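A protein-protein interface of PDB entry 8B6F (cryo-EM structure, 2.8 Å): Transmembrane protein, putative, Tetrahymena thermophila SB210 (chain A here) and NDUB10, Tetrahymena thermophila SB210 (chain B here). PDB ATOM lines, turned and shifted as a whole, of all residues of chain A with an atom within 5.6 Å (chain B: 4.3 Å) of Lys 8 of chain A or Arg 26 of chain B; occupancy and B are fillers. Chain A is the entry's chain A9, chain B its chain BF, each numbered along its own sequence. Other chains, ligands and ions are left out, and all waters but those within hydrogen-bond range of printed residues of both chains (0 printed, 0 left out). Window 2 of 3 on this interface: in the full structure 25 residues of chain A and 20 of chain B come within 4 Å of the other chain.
Printed residues of chain A that touch a printed residue of chain B: Lys 8, Glu 9, Asp 10, Glu 189 and Ile 191. Hydrophobic or aromatic side chains of chain A that line the printed part of chain B: Ile 191. Among the printed residues, 9 pairs touch across the chains. Among the printed residues, Asp or Glu carboxylates within 4 Å of a Lys or Arg side-chain nitrogen of the other chain: Glu 189 of chain A with Arg 26 of chain B (3.5 Å).
Lys 8 of chain A touches one residue of chain B. Arg 26 of chain B touches three residues of chain A. Printed residues of chain A within 4 Å of Ser 27 of chain B: Glu 189 and Ile 191. Of the printed residues of chain B, Ile 191 of chain A touches Arg 7 (3.8 Å) and Ser 27 (3.4 Å). Of the printed residues of chain B, Glu 9 of chain A touches Asn 11 (3.7 Å). The nearest residue of chain A that does not touch Arg 26 of chain B is Glu 9 of chain A (4.1 Å).
O of Leu 3 of chain A sits at hydrogen-bond distance from NZ of Lys 8 of chain A (2.6 Å). NZ of Lys 8 of chain A sits at hydrogen-bond distance from O of Ser 182 of chain A (2.9 Å). The side-chain amino group (NZ) of Lys 8 of chain A lies within hydrogen-bond range of the backbone carbonyl oxygen (O) of Tyr 180 of chain A, 3.2 Å away. The side-chain carboxylate of Glu 189 of chain A lies close to the side-chain carboxylate of Asp 10 of chain A, at 2.6 Å. The backbone carbonyl oxygen (O) of Asp 10 of chain B is in hydrogen-bond range of the backbone NH (N) of Arg 26 of chain B, at 3.1 Å. The side-chain amide oxygen (OD1) of Asn 24 of chain B lies close to the backbone NH (N) of Arg 26 of chain B (3.3 Å).
OD2 of Asp 10 of chain A sits at hydrogen-bond distance from ND2 of Asn 24 of chain B. The side-chain carboxylate of Glu 189 of chain A sits close to the side-chain hydroxyl of Ser 27 of chain B, at 2.3 Å. NH2 of Arg 26 of chain B lies within salt-bridge range of OE2 of Glu 189 of chain A.
Arg 26 of chain B touches Lys 8 of chain A. O of Glu 9 of chain A touches ND2 of Asn 11 of chain B, at 3.7 Å. CB of Asp 10 of chain A touches NH2 of Arg 26 of chain B, 3.6 Å away. Glu 189 of chain A touches Asn 24 of chain B (OE1 to CB, 3.8 Å). Ile 191 of chain A touches Arg 7 of chain B. Ile 191 of chain A touches Ser 27 of chain B (CA to O, 3.4 Å).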
ATOM      1  N   GLU A   2      30.245  22.249  -5.892  1.00  0.00           N
ATOM      2  CA  GLU A   2      28.903  22.530  -5.407  1.00  0.00           C
ATOM      3  C   GLU A   2      28.792  23.998  -5.021  1.00  0.00           C
ATOM      4  O   GLU A   2      29.771  24.627  -4.613  1.00  0.00           O
ATOM      5  CB  GLU A   2      28.530  21.660  -4.198  1.00  0.00           C
ATOM      6  CG  GLU A   2      28.745  20.172  -4.402  1.00  0.00           C
ATOM      7  CD  GLU A   2      30.184  19.756  -4.191  1.00  0.00           C
ATOM      8  OE1 GLU A   2      31.034  20.647  -3.983  1.00  0.00           O
ATOM      9  OE2 GLU A   2      30.465  18.540  -4.229  1.00  0.00           O
ATOM     10  N   LEU A   3      27.584  24.532  -5.157  1.00  0.00           N
ATOM     11  CA  LEU A   3      27.268  25.899  -4.768  1.00  0.00           C
ATOM     12  C   LEU A   3      26.301  25.867  -3.594  1.00  0.00           C
ATOM     13  O   LEU A   3      25.239  25.244  -3.682  1.00  0.00           O
ATOM     14  CB  LEU A   3      26.654  26.679  -5.934  1.00  0.00           C
ATOM     15  CG  LEU A   3      27.503  26.903  -7.190  1.00  0.00           C
ATOM     16  CD1 LEU A   3      27.727  25.619  -7.980  1.00  0.00           C
ATOM     17  CD2 LEU A   3      26.867  27.959  -8.076  1.00  0.00           C
ATOM     18  N   ASN A   4      26.668  26.537  -2.503  1.00  0.00           N
ATOM     19  CA  ASN A   4      25.827  26.596  -1.310  1.00  0.00           C
ATOM     20  C   ASN A   4      25.605  25.195  -0.745  1.00  0.00           C
ATOM     21  O   ASN A   4      24.480  24.774  -0.477  1.00  0.00           O
ATOM     22  CB  ASN A   4      24.496  27.282  -1.623  1.00  0.00           C
ATOM     23  CG  ASN A   4      23.721  27.656  -0.377  1.00  0.00           C
ATOM     24  OD1 ASN A   4      24.286  27.773   0.709  1.00  0.00           O
ATOM     25  ND2 ASN A   4      22.417  27.849  -0.530  1.00  0.00           N
ATOM     26  N   SER A   5      26.709  24.468  -0.561  1.00  0.00           N
ATOM     27  CA  SER A   5      26.617  23.087  -0.103  1.00  0.00           C
ATOM     28  C   SER A   5      26.006  23.003   1.288  1.00  0.00           C
ATOM     29  O   SER A   5      25.188  22.119   1.563  1.00  0.00           O
ATOM     30  CB  SER A   5      28.005  22.446  -0.116  1.00  0.00           C
ATOM     31  OG  SER A   5      27.947  21.090   0.295  1.00  0.00           O
ATOM     32  N   SER A   6      26.392  23.915   2.182  1.00  0.00           N
ATOM     33  CA  SER A   6      25.945  23.825   3.568  1.00  0.00           C
ATOM     34  C   SER A   6      24.428  23.917   3.674  1.00  0.00           C
ATOM     35  O   SER A   6      23.802  23.140   4.403  1.00  0.00           O
ATOM     36  CB  SER A   6      26.604  24.928   4.395  1.00  0.00           C
ATOM     37  OG  SER A   6      26.149  24.902   5.738  1.00  0.00           O
ATOM     38  N   ALA A   7      23.818  24.855   2.948  1.00  0.00           N
ATOM     39  CA  ALA A   7      22.382  25.070   3.083  1.00  0.00           C
ATOM     40  C   ALA A   7      21.590  23.839   2.667  1.00  0.00           C
ATOM     41  O   ALA A   7      20.646  23.438   3.358  1.00  0.00           O
ATOM     42  CB  ALA A   7      21.953  26.281   2.256  1.00  0.00           C
ATOM     43  N   LYS A   8      21.955  23.225   1.545  1.00  0.00           N
ATOM     44  CA  LYS A   8      21.211  22.084   1.014  1.00  0.00           C
ATOM     45  C   LYS A   8      21.881  20.783   1.447  1.00  0.00           C
ATOM     46  O   LYS A   8      22.486  20.052   0.664  1.00  0.00           O
ATOM     47  CB  LYS A   8      21.088  22.192  -0.505  1.00  0.00           C
ATOM     48  CG  LYS A   8      22.407  22.260  -1.254  1.00  0.00           C
ATOM     49  CD  LYS A   8      22.207  22.830  -2.650  1.00  0.00           C
ATOM     50  CE  LYS A   8      23.512  22.859  -3.421  1.00  0.00           C
ATOM     51  NZ  LYS A   8      23.395  23.639  -4.682  1.00  0.00           N
ATOM     52  N   GLU A   9      21.748  20.504   2.740  1.00  0.00           N
ATOM     53  CA  GLU A   9      22.258  19.289   3.355  1.00  0.00           C
ATOM     54  C   GLU A   9      21.111  18.557   4.033  1.00  0.00           C
ATOM     55  O   GLU A   9      20.268  19.177   4.687  1.00  0.00           O
ATOM     56  CB  GLU A   9      23.353  19.600   4.381  1.00  0.00           C
ATOM     57  CG  GLU A   9      23.873  18.375   5.125  1.00  0.00           C
ATOM     58  CD  GLU A   9      24.784  18.738   6.279  1.00  0.00           C
ATOM     59  OE1 GLU A   9      25.179  19.918   6.373  1.00  0.00           O
ATOM     60  OE2 GLU A   9      25.101  17.848   7.094  1.00  0.00           O
ATOM     61  N   ASP A  10      21.085  17.237   3.875  1.00  0.00           N
ATOM     62  CA  ASP A  10      20.081  16.396   4.522  1.00  0.00           C
ATOM     63  C   ASP A  10      20.650  15.941   5.858  1.00  0.00           C
ATOM     64  O   ASP A  10      21.411  14.974   5.926  1.00  0.00           O
ATOM     65  CB  ASP A  10      19.710  15.215   3.635  1.00  0.00           C
ATOM     66  CG  ASP A  10      18.490  14.473   4.138  1.00  0.00           C
ATOM     67  OD1 ASP A  10      18.004  14.807   5.238  1.00  0.00           O
ATOM     68  OD2 ASP A  10      18.013  13.559   3.435  1.00  0.00           O
ATOM     69  N   PHE A 179      20.604  26.152  -9.582  1.00  0.00           N
ATOM     70  CA  PHE A 179      21.914  25.589  -9.286  1.00  0.00           C
ATOM     71  C   PHE A 179      22.544  26.101  -7.997  1.00  0.00           C
ATOM     72  O   PHE A 179      23.687  25.736  -7.704  1.00  0.00           O
ATOM     73  CB  PHE A 179      22.872  25.848 -10.456  1.00  0.00           C
ATOM     74  CG  PHE A 179      22.476  25.145 -11.720  1.00  0.00           C
ATOM     75  CD1 PHE A 179      22.478  23.763 -11.788  1.00  0.00           C
ATOM     76  CD2 PHE A 179      22.117  25.864 -12.844  1.00  0.00           C
ATOM     77  CE1 PHE A 179      22.115  23.113 -12.949  1.00  0.00           C
ATOM     78  CE2 PHE A 179      21.753  25.220 -14.006  1.00  0.00           C
ATOM     79  CZ  PHE A 179      21.754  23.844 -14.061  1.00  0.00           C
ATOM     80  N   TYR A 180      21.844  26.925  -7.219  1.00  0.00           N
ATOM     81  CA  TYR A 180      22.364  27.437  -5.956  1.00  0.00           C
ATOM     82  C   TYR A 180      21.530  26.978  -4.771  1.00  0.00           C
ATOM     83  O   TYR A 180      22.080  26.444  -3.802  1.00  0.00           O
ATOM     84  CB  TYR A 180      22.427  28.974  -5.991  1.00  0.00           C
ATOM     85  CG  TYR A 180      23.121  29.599  -4.802  1.00  0.00           C
ATOM     86  CD1 TYR A 180      24.496  29.788  -4.795  1.00  0.00           C
ATOM     87  CD2 TYR A 180      22.396  30.018  -3.695  1.00  0.00           C
ATOM     88  CE1 TYR A 180      25.132  30.366  -3.713  1.00  0.00           C
ATOM     89  CE2 TYR A 180      23.022  30.597  -2.608  1.00  0.00           C
ATOM     90  CZ  TYR A 180      24.390  30.769  -2.624  1.00  0.00           C
ATOM     91  OH  TYR A 180      25.016  31.345  -1.544  1.00  0.00           O
ATOM     92  N   ASN A 181      20.215  27.175  -4.821  1.00  0.00           N
ATOM     93  CA  ASN A 181      19.316  26.685  -3.786  1.00  0.00           C
ATOM     94  C   ASN A 181      18.890  25.240  -4.012  1.00  0.00           C
ATOM     95  O   ASN A 181      18.276  24.645  -3.120  1.00  0.00           O
ATOM     96  CB  ASN A 181      18.070  27.571  -3.702  1.00  0.00           C
ATOM     97  CG  ASN A 181      18.409  29.027  -3.476  1.00  0.00           C
ATOM     98  OD1 ASN A 181      18.064  29.888  -4.284  1.00  0.00           O
ATOM     99  ND2 ASN A 181      19.088  29.312  -2.371  1.00  0.00           N
ATOM    100  N   SER A 182      19.199  24.669  -5.172  1.00  0.00           N
ATOM    101  CA  SER A 182      18.830  23.304  -5.505  1.00  0.00           C
ATOM    102  C   SER A 182      20.073  22.539  -5.932  1.00  0.00           C
ATOM    103  O   SER A 182      21.063  23.121  -6.380  1.00  0.00           O
ATOM    104  CB  SER A 182      17.780  23.258  -6.623  1.00  0.00           C
ATOM    105  OG  SER A 182      16.608  23.962  -6.255  1.00  0.00           O
ATOM    106  N   SER A 183      20.009  21.223  -5.783  1.00  0.00           N
ATOM    107  CA  SER A 183      21.134  20.334  -6.052  1.00  0.00           C
ATOM    108  C   SER A 183      20.786  19.475  -7.265  1.00  0.00           C
ATOM    109  O   SER A 183      20.214  18.393  -7.134  1.00  0.00           O
ATOM    110  CB  SER A 183      21.439  19.483  -4.825  1.00  0.00           C
ATOM    111  OG  SER A 183      22.525  18.611  -5.069  1.00  0.00           O
ATOM    112  N   GLN A 186      24.863  18.450  -7.916  1.00  0.00           N
ATOM    113  CA  GLN A 186      25.552  18.346  -6.637  1.00  0.00           C
ATOM    114  C   GLN A 186      24.924  17.274  -5.755  1.00  0.00           C
ATOM    115  O   GLN A 186      24.927  17.391  -4.530  1.00  0.00           O
ATOM    116  CB  GLN A 186      25.547  19.690  -5.908  1.00  0.00           C
ATOM    117  CG  GLN A 186      25.978  20.882  -6.749  1.00  0.00           C
ATOM    118  CD  GLN A 186      24.881  21.393  -7.659  1.00  0.00           C
ATOM    119  OE1 GLN A 186      23.985  20.646  -8.052  1.00  0.00           O
ATOM    120  NE2 GLN A 186      24.938  22.675  -7.990  1.00  0.00           N
ATOM    121  N   GLU A 189      22.895  12.183  -2.515  1.00  0.00           N
ATOM    122  CA  GLU A 189      22.047  11.053  -2.177  1.00  0.00           C
ATOM    123  C   GLU A 189      21.709  10.293  -3.449  1.00  0.00           C
ATOM    124  O   GLU A 189      21.571  10.884  -4.523  1.00  0.00           O
ATOM    125  CB  GLU A 189      20.753  11.497  -1.488  1.00  0.00           C
ATOM    126  CG  GLU A 189      20.970  12.345  -0.252  1.00  0.00           C
ATOM    127  CD  GLU A 189      19.669  12.838   0.345  1.00  0.00           C
ATOM    128  OE1 GLU A 189      18.613  12.663  -0.298  1.00  0.00           O
ATOM    129  OE2 GLU A 189      19.701  13.400   1.457  1.00  0.00           O
ATOM    130  N   ILE A 191      19.271   8.359  -5.942  1.00  0.00           N
ATOM    131  CA  ILE A 191      17.861   8.511  -6.275  1.00  0.00           C
ATOM    132  C   ILE A 191      17.110   7.257  -5.855  1.00  0.00           C
ATOM    133  O   ILE A 191      17.488   6.134  -6.214  1.00  0.00           O
ATOM    134  CB  ILE A 191      17.686   8.799  -7.776  1.00  0.00           C
ATOM    135  CG1 ILE A 191      18.046  10.253  -8.102  1.00  0.00           C
ATOM    136  CG2 ILE A 191      16.256   8.520  -8.233  1.00  0.00           C
ATOM    137  CD1 ILE A 191      19.515  10.597  -7.951  1.00  0.00           C
ATOM    138  N   ARG B   7      12.156  15.256 -11.860  1.00  0.00           N
ATOM    139  CA  ARG B   7      13.045  15.429 -10.722  1.00  0.00           C
ATOM    140  C   ARG B   7      12.541  16.550  -9.824  1.00  0.00           C
ATOM    141  O   ARG B   7      12.128  17.611 -10.298  1.00  0.00           O
ATOM    142  CB  ARG B   7      14.464  15.735 -11.203  1.00  0.00           C
ATOM    143  CG  ARG B   7      15.494  15.866 -10.089  1.00  0.00           C
ATOM    144  CD  ARG B   7      15.707  14.554  -9.350  1.00  0.00           C
ATOM    145  NE  ARG B   7      16.217  13.507 -10.228  1.00  0.00           N
ATOM    146  CZ  ARG B   7      17.501  13.304 -10.490  1.00  0.00           C
ATOM    147  NH1 ARG B   7      18.445  14.064  -9.962  1.00  0.00           N
ATOM    148  NH2 ARG B   7      17.847  12.309 -11.303  1.00  0.00           N
ATOM    149  N   GLN B   8      12.578  16.306  -8.522  1.00  0.00           N
ATOM    150  CA  GLN B   8      12.103  17.258  -7.533  1.00  0.00           C
ATOM    151  C   GLN B   8      13.273  18.033  -6.943  1.00  0.00           C
ATOM    152  O   GLN B   8      14.395  17.529  -6.857  1.00  0.00           O
ATOM    153  CB  GLN B   8      11.341  16.539  -6.419  1.00  0.00           C
ATOM    154  CG  GLN B   8      10.099  15.811  -6.901  1.00  0.00           C
ATOM    155  CD  GLN B   8       9.033  16.752  -7.418  1.00  0.00           C
ATOM    156  OE1 GLN B   8       9.015  17.933  -7.078  1.00  0.00           O
ATOM    157  NE2 GLN B   8       8.138  16.233  -8.249  1.00  0.00           N
ATOM    158  N   ASP B  10      12.658  20.199  -3.938  1.00  0.00           N
ATOM    159  CA  ASP B  10      12.428  20.473  -2.527  1.00  0.00           C
ATOM    160  C   ASP B  10      13.266  19.544  -1.657  1.00  0.00           C
ATOM    161  O   ASP B  10      13.518  18.387  -2.005  1.00  0.00           O
ATOM    162  CB  ASP B  10      10.946  20.304  -2.196  1.00  0.00           C
ATOM    163  CG  ASP B  10      10.604  20.766  -0.794  1.00  0.00           C
ATOM    164  OD1 ASP B  10      11.487  21.341  -0.125  1.00  0.00           O
ATOM    165  OD2 ASP B  10       9.452  20.551  -0.360  1.00  0.00           O
ATOM    166  N   ASN B  11      13.699  20.063  -0.508  1.00  0.00           N
ATOM    167  CA  ASN B  11      14.531  19.322   0.430  1.00  0.00           C
ATOM    168  C   ASN B  11      13.743  18.845   1.648  1.00  0.00           C
ATOM    169  O   ASN B  11      14.300  18.724   2.743  1.00  0.00           O
ATOM    170  CB  ASN B  11      15.715  20.187   0.864  1.00  0.00           C
ATOM    171  CG  ASN B  11      16.764  19.404   1.628  1.00  0.00           C
ATOM    172  OD1 ASN B  11      16.810  18.178   1.560  1.00  0.00           O
ATOM    173  ND2 ASN B  11      17.615  20.113   2.361  1.00  0.00           N
ATOM    174  N   ASN B  24      13.347  11.468   1.036  1.00  0.00           N
ATOM    175  CA  ASN B  24      13.520  12.893   0.812  1.00  0.00           C
ATOM    176  C   ASN B  24      12.877  13.259  -0.516  1.00  0.00           C
ATOM    177  O   ASN B  24      12.933  12.484  -1.475  1.00  0.00           O
ATOM    178  CB  ASN B  24      15.002  13.278   0.819  1.00  0.00           C
ATOM    179  CG  ASN B  24      15.216  14.771   0.938  1.00  0.00           C
ATOM    180  OD1 ASN B  24      14.480  15.562   0.356  1.00  0.00           O
ATOM    181  ND2 ASN B  24      16.225  15.163   1.706  1.00  0.00           N
ATOM    182  N   THR B  25      12.258  14.440  -0.568  1.00  0.00           N
ATOM    183  CA  THR B  25      11.499  14.821  -1.754  1.00  0.00           C
ATOM    184  C   THR B  25      12.387  14.873  -2.989  1.00  0.00           C
ATOM    185  O   THR B  25      11.992  14.413  -4.067  1.00  0.00           O
ATOM    186  CB  THR B  25      10.818  16.170  -1.531  1.00  0.00           C
ATOM    187  OG1 THR B  25       9.984  16.098  -0.370  1.00  0.00           O
ATOM    188  CG2 THR B  25       9.965  16.547  -2.735  1.00  0.00           C
ATOM    189  N   ARG B  26      13.588  15.435  -2.857  1.00  0.00           N
ATOM    190  CA  ARG B  26      14.484  15.552  -4.000  1.00  0.00           C
ATOM    191  C   ARG B  26      15.032  14.205  -4.455  1.00  0.00           C
ATOM    192  O   ARG B  26      15.471  14.090  -5.603  1.00  0.00           O
ATOM    193  CB  ARG B  26      15.640  16.494  -3.661  1.00  0.00           C
ATOM    194  CG  ARG B  26      16.503  16.025  -2.505  1.00  0.00           C
ATOM    195  CD  ARG B  26      17.573  17.047  -2.165  1.00  0.00           C
ATOM    196  NE  ARG B  26      18.442  16.578  -1.096  1.00  0.00           N
ATOM    197  CZ  ARG B  26      19.412  17.294  -0.545  1.00  0.00           C
ATOM    198  NH1 ARG B  26      19.664  18.531  -0.937  1.00  0.00           N
ATOM    199  NH2 ARG B  26      20.143  16.759   0.426  1.00  0.00           N
ATOM    200  N   SER B  27      15.020  13.192  -3.593  1.00  0.00           N
ATOM    201  CA  SER B  27      15.613  11.898  -3.906  1.00  0.00           C
ATOM    202  C   SER B  27      14.615  10.888  -4.457  1.00  0.00           C
ATOM    203  O   SER B  27      15.022   9.787  -4.834  1.00  0.00           O
ATOM    204  CB  SER B  27      16.275  11.312  -2.657  1.00  0.00           C
ATOM    205  OG  SER B  27      17.294  12.168  -2.171  1.00  0.00           O
ATOM    206  N   LEU B  28      13.330  11.224  -4.515  1.00  0.00           N
ATOM    207  CA  LEU B  28      12.333  10.267  -4.969  1.00  0.00           C
ATOM    208  C   LEU B  28      12.549   9.910  -6.434  1.00  0.00           C
ATOM    209  O   LEU B  28      12.885  10.765  -7.256  1.00  0.00           O
ATOM    210  CB  LEU B  28      10.928  10.837  -4.786  1.00  0.00           C
ATOM    211  CG  LEU B  28      10.543  11.284  -3.378  1.00  0.00           C
ATOM    212  CD1 LEU B  28       9.116  11.797  -3.381  1.00  0.00           C
ATOM    213  CD2 LEU B  28      10.707  10.154  -2.378  1.00  0.00           C
